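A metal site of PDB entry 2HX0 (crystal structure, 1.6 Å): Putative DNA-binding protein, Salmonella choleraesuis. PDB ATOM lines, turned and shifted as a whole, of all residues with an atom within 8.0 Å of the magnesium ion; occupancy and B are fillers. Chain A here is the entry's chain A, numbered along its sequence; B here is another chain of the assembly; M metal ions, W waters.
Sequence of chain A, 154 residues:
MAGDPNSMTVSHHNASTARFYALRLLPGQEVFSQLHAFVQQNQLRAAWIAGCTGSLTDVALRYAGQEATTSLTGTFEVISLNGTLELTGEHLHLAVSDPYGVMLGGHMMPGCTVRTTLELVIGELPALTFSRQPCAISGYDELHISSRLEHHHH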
ATOM      1  N   ARG A  62      17.079 -14.670  22.634  1.00  0.00           N
ATOM      2  CA  ARG A  62      15.666 -14.327  22.756  1.00  0.00           C
ATOM      3  C   ARG A  62      14.988 -15.316  21.829  1.00  0.00           C
ATOM      4  O   ARG A  62      15.159 -15.248  20.608  1.00  0.00           O
ATOM      5  CB  ARG A  62      15.412 -12.891  22.281  1.00  0.00           C
ATOM      6  CG  ARG A  62      14.003 -12.402  22.563  1.00  0.00           C
ATOM      7  CD  ARG A  62      13.806 -10.975  22.076  1.00  0.00           C
ATOM      8  NE  ARG A  62      13.854 -10.900  20.621  1.00  0.00           N
ATOM      9  CZ  ARG A  62      13.775  -9.772  19.915  1.00  0.00           C
ATOM     10  NH1 ARG A  62      13.638  -8.610  20.539  1.00  0.00           N
ATOM     11  NH2 ARG A  62      13.821  -9.806  18.592  1.00  0.00           N
ATOM     12  N   ALA A  64      12.052 -17.448  19.697  1.00  0.00           N
ATOM     13  CA  ALA A  64      10.989 -17.074  18.787  1.00  0.00           C
ATOM     14  C   ALA A  64       9.722 -16.544  19.448  1.00  0.00           C
ATOM     15  O   ALA A  64       9.110 -17.217  20.276  1.00  0.00           O
ATOM     16  CB  ALA A  64      10.644 -18.252  17.876  1.00  0.00           C
ATOM     17  N   ASN A  82      24.444 -15.787  12.212  1.00  0.00           N
ATOM     18  CA  ASN A  82      24.057 -15.184  10.948  1.00  0.00           C
ATOM     19  C   ASN A  82      23.312 -13.883  11.117  1.00  0.00           C
ATOM     20  O   ASN A  82      22.705 -13.626  12.154  1.00  0.00           O
ATOM     21  CB  ASN A  82      23.178 -16.162  10.156  1.00  0.00           C
ATOM     22  CG  ASN A  82      23.963 -17.290   9.547  1.00  0.00           C
ATOM     23  OD1 ASN A  82      24.800 -17.065   8.658  1.00  0.00           O
ATOM     24  ND2 ASN A  82      23.713 -18.512   9.996  1.00  0.00           N
ATOM     25  N   GLU A  90      21.460  -3.834  13.772  1.00  0.00           N
ATOM     26  CA  GLU A  90      21.853  -5.189  13.436  1.00  0.00           C
ATOM     27  C   GLU A  90      20.686  -6.137  13.640  1.00  0.00           C
ATOM     28  O   GLU A  90      19.666  -5.767  14.221  1.00  0.00           O
ATOM     29  CB  GLU A  90      23.024  -5.654  14.316  1.00  0.00           C
ATOM     30  CG  GLU A  90      22.667  -5.929  15.781  1.00  0.00           C
ATOM     31  CD  GLU A  90      22.390  -4.661  16.561  1.00  0.00           C
ATOM     32  OE1 GLU A  90      23.213  -3.724  16.476  1.00  0.00           O
ATOM     33  OE2 GLU A  90      21.364  -4.601  17.276  1.00  0.00           O
ATOM     34  N   HIS A  91      20.832  -7.361  13.151  1.00  0.00           N
ATOM     35  CA  HIS A  91      19.820  -8.407  13.292  1.00  0.00           C
ATOM     36  C   HIS A  91      20.611  -9.694  13.182  1.00  0.00           C
ATOM     37  O   HIS A  91      20.923 -10.138  12.071  1.00  0.00           O
ATOM     38  CB  HIS A  91      18.770  -8.305  12.184  1.00  0.00           C
ATOM     39  CG  HIS A  91      17.587  -9.207  12.402  1.00  0.00           C
ATOM     40  ND1 HIS A  91      16.502  -9.232  11.551  1.00  0.00           N
ATOM     41  CD2 HIS A  91      17.323 -10.107  13.375  1.00  0.00           C
ATOM     42  CE1 HIS A  91      15.613 -10.118  11.995  1.00  0.00           C
ATOM     43  NE2 HIS A  91      16.095 -10.657  13.097  1.00  0.00           N
ATOM     44  N   LEU A  92      20.936 -10.284  14.322  1.00  0.00           N
ATOM     45  CA  LEU A  92      21.737 -11.501  14.358  1.00  0.00           C
ATOM     46  C   LEU A  92      21.064 -12.665  15.077  1.00  0.00           C
ATOM     47  O   LEU A  92      20.452 -12.477  16.127  1.00  0.00           O
ATOM     48  CB  LEU A  92      23.083 -11.216  15.034  1.00  0.00           C
ATOM     49  CG  LEU A  92      23.897 -10.078  14.408  1.00  0.00           C
ATOM     50  CD1 LEU A  92      25.008  -9.640  15.349  1.00  0.00           C
ATOM     51  CD2 LEU A  92      24.452 -10.533  13.085  1.00  0.00           C
ATOM     52  N   HIS A  93      21.188 -13.857  14.509  1.00  0.00           N
ATOM     53  CA  HIS A  93      20.639 -15.063  15.101  1.00  0.00           C
ATOM     54  C   HIS A  93      21.792 -15.991  15.415  1.00  0.00           C
ATOM     55  O   HIS A  93      22.762 -16.059  14.668  1.00  0.00           O
ATOM     56  CB  HIS A  93      19.637 -15.737  14.154  1.00  0.00           C
ATOM     57  CG  HIS A  93      18.324 -15.017  14.073  1.00  0.00           C
ATOM     58  ND1 HIS A  93      17.281 -15.457  13.284  1.00  0.00           N
ATOM     59  CD2 HIS A  93      17.876 -13.911  14.710  1.00  0.00           C
ATOM     60  CE1 HIS A  93      16.244 -14.646  13.436  1.00  0.00           C
ATOM     61  NE2 HIS A  93      16.578 -13.696  14.290  1.00  0.00           N
ATOM     62  N   GLY A 106      18.198 -18.892  18.536  1.00  0.00           N
ATOM     63  CA  GLY A 106      17.315 -17.766  18.742  1.00  0.00           C
ATOM     64  C   GLY A 106      17.938 -16.456  18.292  1.00  0.00           C
ATOM     65  O   GLY A 106      18.982 -16.439  17.659  1.00  0.00           O
ATOM     66  N   HIS A 107      17.262 -15.366  18.630  1.00  0.00           N
ATOM     67  CA  HIS A 107      17.715 -14.024  18.297  1.00  0.00           C
ATOM     68  C   HIS A 107      18.837 -13.715  19.286  1.00  0.00           C
ATOM     69  O   HIS A 107      18.645 -13.794  20.498  1.00  0.00           O
ATOM     70  CB  HIS A 107      16.536 -13.052  18.487  1.00  0.00           C
ATOM     71  CG  HIS A 107      16.832 -11.637  18.089  1.00  0.00           C
ATOM     72  ND1 HIS A 107      16.978 -11.248  16.783  1.00  0.00           N
ATOM     73  CD2 HIS A 107      16.955 -10.508  18.842  1.00  0.00           C
ATOM     74  CE1 HIS A 107      17.178  -9.937  16.737  1.00  0.00           C
ATOM     75  NE2 HIS A 107      17.170  -9.469  17.968  1.00  0.00           N
ATOM     76  N   MET A 108      20.032 -13.384  18.777  1.00  0.00           N
ATOM     77  CA  MET A 108      21.151 -13.101  19.665  1.00  0.00           C
ATOM     78  C   MET A 108      20.987 -11.773  20.383  1.00  0.00           C
ATOM     79  O   MET A 108      20.609 -10.762  19.782  1.00  0.00           O
ATOM     80  CB  MET A 108      22.455 -13.102  18.871  1.00  0.00           C
ATOM     81  CG  MET A 108      23.683 -12.957  19.749  1.00  0.00           C
ATOM     82  SD  MET A 108      25.311 -13.302  18.769  1.00  0.00           S
ATOM     83  CE  MET A 108      25.833 -11.499  18.375  1.00  0.00           C
ATOM     84  N   GLU A 142      12.453  -2.495  10.164  1.00  0.00           N
ATOM     85  CA  GLU A 142      13.027  -3.579   9.365  1.00  0.00           C
ATOM     86  C   GLU A 142      14.151  -3.100   8.465  1.00  0.00           C
ATOM     87  O   GLU A 142      14.331  -1.906   8.260  1.00  0.00           O
ATOM     88  CB  GLU A 142      11.930  -4.222   8.511  1.00  0.00           C
ATOM     89  CG  GLU A 142      10.725  -4.712   9.313  1.00  0.00           C
ATOM     90  CD  GLU A 142      11.043  -5.896  10.204  1.00  0.00           C
ATOM     91  OE1 GLU A 142      12.182  -6.391  10.159  1.00  0.00           O
ATOM     92  OE2 GLU A 142      10.136  -6.334  10.948  1.00  0.00           O
ATOM     93  N   THR B  53      18.723 -14.184   7.797  1.00  0.00           N
ATOM     94  CA  THR B  53      18.142 -14.104   9.137  1.00  0.00           C
ATOM     95  C   THR B  53      16.706 -13.677   8.969  1.00  0.00           C
ATOM     96  O   THR B  53      16.357 -12.992   8.014  1.00  0.00           O
ATOM     97  CB  THR B  53      18.883 -13.087  10.012  1.00  0.00           C
ATOM     98  OG1 THR B  53      18.348 -13.142  11.344  1.00  0.00           O
ATOM     99  CG2 THR B  53      18.725 -11.677   9.464  1.00  0.00           C
ATOM    100  N   GLY B  54      15.837 -14.103   9.886  1.00  0.00           N
ATOM    101  CA  GLY B  54      14.445 -13.732   9.777  1.00  0.00           C
ATOM    102  C   GLY B  54      13.540 -14.617  10.602  1.00  0.00           C
ATOM    103  O   GLY B  54      13.986 -15.310  11.514  1.00  0.00           O
ATOM    104  N   SER B  55      12.256 -14.590  10.271  1.00  0.00           N
ATOM    105  CA  SER B  55      11.249 -15.352  10.994  1.00  0.00           C
ATOM    106  C   SER B  55      10.225 -15.956  10.033  1.00  0.00           C
ATOM    107  O   SER B  55       9.967 -15.405   8.967  1.00  0.00           O
ATOM    108  CB  SER B  55      10.547 -14.436  11.993  1.00  0.00           C
ATOM    109  OG  SER B  55      10.061 -13.274  11.353  1.00  0.00           O
ATOM    110  N   PHE B  76       8.464 -19.284  14.333  1.00  0.00           N
ATOM    111  CA  PHE B  76       9.832 -19.752  14.190  1.00  0.00           C
ATOM    112  C   PHE B  76      10.821 -18.669  13.794  1.00  0.00           C
ATOM    113  O   PHE B  76      10.461 -17.686  13.151  1.00  0.00           O
ATOM    114  CB  PHE B  76       9.922 -20.853  13.133  1.00  0.00           C
ATOM    115  CG  PHE B  76       9.073 -22.055  13.422  1.00  0.00           C
ATOM    116  CD1 PHE B  76       7.752 -22.116  12.973  1.00  0.00           C
ATOM    117  CD2 PHE B  76       9.597 -23.150  14.102  1.00  0.00           C
ATOM    118  CE1 PHE B  76       6.968 -23.255  13.197  1.00  0.00           C
ATOM    119  CE2 PHE B  76       8.842 -24.285  14.335  1.00  0.00           C
ATOM    120  CZ  PHE B  76       7.513 -24.339  13.871  1.00  0.00           C
ATOM    121  N   GLU B  77      12.076 -18.875  14.189  1.00  0.00           N
ATOM    122  CA  GLU B  77      13.145 -17.964  13.822  1.00  0.00           C
ATOM    123  C   GLU B  77      13.984 -18.736  12.822  1.00  0.00           C
ATOM    124  O   GLU B  77      14.209 -19.936  12.983  1.00  0.00           O
ATOM    125  CB  GLU B  77      14.011 -17.598  15.022  1.00  0.00           C
ATOM    126  CG  GLU B  77      13.316 -16.753  16.069  1.00  0.00           C
ATOM    127  CD  GLU B  77      12.938 -15.397  15.540  1.00  0.00           C
ATOM    128  OE1 GLU B  77      13.840 -14.618  15.194  1.00  0.00           O
ATOM    129  OE2 GLU B  77      11.724 -15.103  15.462  1.00  0.00           O
ATOM    130  N   VAL B  78      14.435 -18.055  11.777  1.00  0.00           N
ATOM    131  CA  VAL B  78      15.290 -18.708  10.802  1.00  0.00           C
ATOM    132  C   VAL B  78      16.702 -18.607  11.337  1.00  0.00           C
ATOM    133  O   VAL B  78      17.246 -17.509  11.507  1.00  0.00           O
ATOM    134  CB  VAL B  78      15.213 -18.023   9.426  1.00  0.00           C
ATOM    135  CG1 VAL B  78      16.277 -18.616   8.502  1.00  0.00           C
ATOM    136  CG2 VAL B  78      13.838 -18.210   8.828  1.00  0.00           C
ATOM    137  N   ARG B 115       7.224 -14.425   8.515  1.00  0.00           N
ATOM    138  CA  ARG B 115       6.410 -13.940   9.616  1.00  0.00           C
ATOM    139  C   ARG B 115       6.525 -12.421   9.691  1.00  0.00           C
ATOM    140  O   ARG B 115       5.561 -11.705   9.420  1.00  0.00           O
ATOM    141  CB  ARG B 115       6.849 -14.587  10.925  1.00  0.00           C
ATOM    142  CG  ARG B 115       5.948 -14.275  12.115  1.00  0.00           C
ATOM    143  CD  ARG B 115       5.965 -15.415  13.129  1.00  0.00           C
ATOM    144  NE  ARG B 115       7.308 -15.697  13.641  1.00  0.00           N
ATOM    145  CZ  ARG B 115       7.937 -14.936  14.531  1.00  0.00           C
ATOM    146  NH1 ARG B 115       7.360 -13.842  15.004  1.00  0.00           N
ATOM    147  NH2 ARG B 115       9.157 -15.268  14.943  1.00  0.00           N
ATOM    148  N   THR B 116       7.709 -11.924  10.058  1.00  0.00           N
ATOM    149  CA  THR B 116       7.926 -10.485  10.137  1.00  0.00           C
ATOM    150  C   THR B 116       8.920 -10.019   9.087  1.00  0.00           C
ATOM    151  O   THR B 116       8.801  -8.900   8.569  1.00  0.00           O
ATOM    152  CB  THR B 116       8.447 -10.045  11.529  1.00  0.00           C
ATOM    153  OG1 THR B 116       9.727 -10.635  11.775  1.00  0.00           O
ATOM    154  CG2 THR B 116       7.473 -10.466  12.617  1.00  0.00           C
ATOM    155  N   THR B 117       9.882 -10.856   8.738  1.00  0.00           N
ATOM    156  CA  THR B 117      10.888 -10.468   7.765  1.00  0.00           C
ATOM    157  C   THR B 117      11.836 -11.616   7.421  1.00  0.00           C
ATOM    158  O   THR B 117      11.919 -12.606   8.145  1.00  0.00           O
ATOM    159  CB  THR B 117      11.767  -9.309   8.320  1.00  0.00           C
ATOM    160  OG1 THR B 117      12.549  -8.741   7.265  1.00  0.00           O
ATOM    161  CG2 THR B 117      12.719  -9.833   9.382  1.00  0.00           C
ATOM    162  N   GLU B 119      15.762 -11.470   5.874  1.00  0.00           N
ATOM    163  CA  GLU B 119      16.869 -10.683   5.335  1.00  0.00           C
ATOM    164  C   GLU B 119      17.846 -11.633   4.673  1.00  0.00           C
ATOM    165  O   GLU B 119      18.266 -12.605   5.278  1.00  0.00           O
ATOM    166  CB  GLU B 119      17.551  -9.907   6.456  1.00  0.00           C
ATOM    167  CG  GLU B 119      16.661  -8.833   7.064  1.00  0.00           C
ATOM    168  CD  GLU B 119      17.243  -8.224   8.329  1.00  0.00           C
ATOM    169  OE1 GLU B 119      18.476  -8.086   8.420  1.00  0.00           O
ATOM    170  OE2 GLU B 119      16.464  -7.869   9.238  1.00  0.00           O
HETATM  171 MG    MG M   1      15.483 -11.864  14.805  1.00  0.00          MG
HETATM  172  O   HOH W   1      13.495 -12.223  13.298  1.00  0.00           O
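A ring nitrogen (ND1) of His 91 lies within hydrogen-bond range of the side-chain carboxylate (OE2) of Glu 119 of chain B (2.7 Å). OE1 of Glu 77 of chain B lies close to NE2 of His 93 (3.0 Å). A ring nitrogen (ND1) of His 93 is in hydrogen-bond range of the side-chain hydroxyl (OG1) of Thr 53 of chain B (3.2 Å). ND1 of His 93 lies within hydrogen-bond range of O of Val 78 of chain B (2.7 Å). The backbone NH of His 93 lies within hydrogen-bond range of the backbone carbonyl oxygen of Asn 82 (2.8 Å). The backbone NH (N) of Arg 62 lies within hydrogen-bond range of the backbone carbonyl oxygen (O) of His 107. The side-chain carboxylate of Glu 77 of chain B lies within salt-bridge range of the guanidinium group of Arg 115 of chain B.
Merely in contact with the magnesium ion: Glu 77 of chain B. Of the 21 residues printed, 4 come within 4 Å of the magnesium ion.
NE2 of His 91 binds the magnesium ion (2.2 Å). NE2 of His 93 binds the magnesium ion (2.2 Å). Water W1 is bound to the magnesium ion (2.5 Å). The magnesium ion is bound by a ring nitrogen (ND1) of His 107. The magnesium ion has four donor atoms within binding distance.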
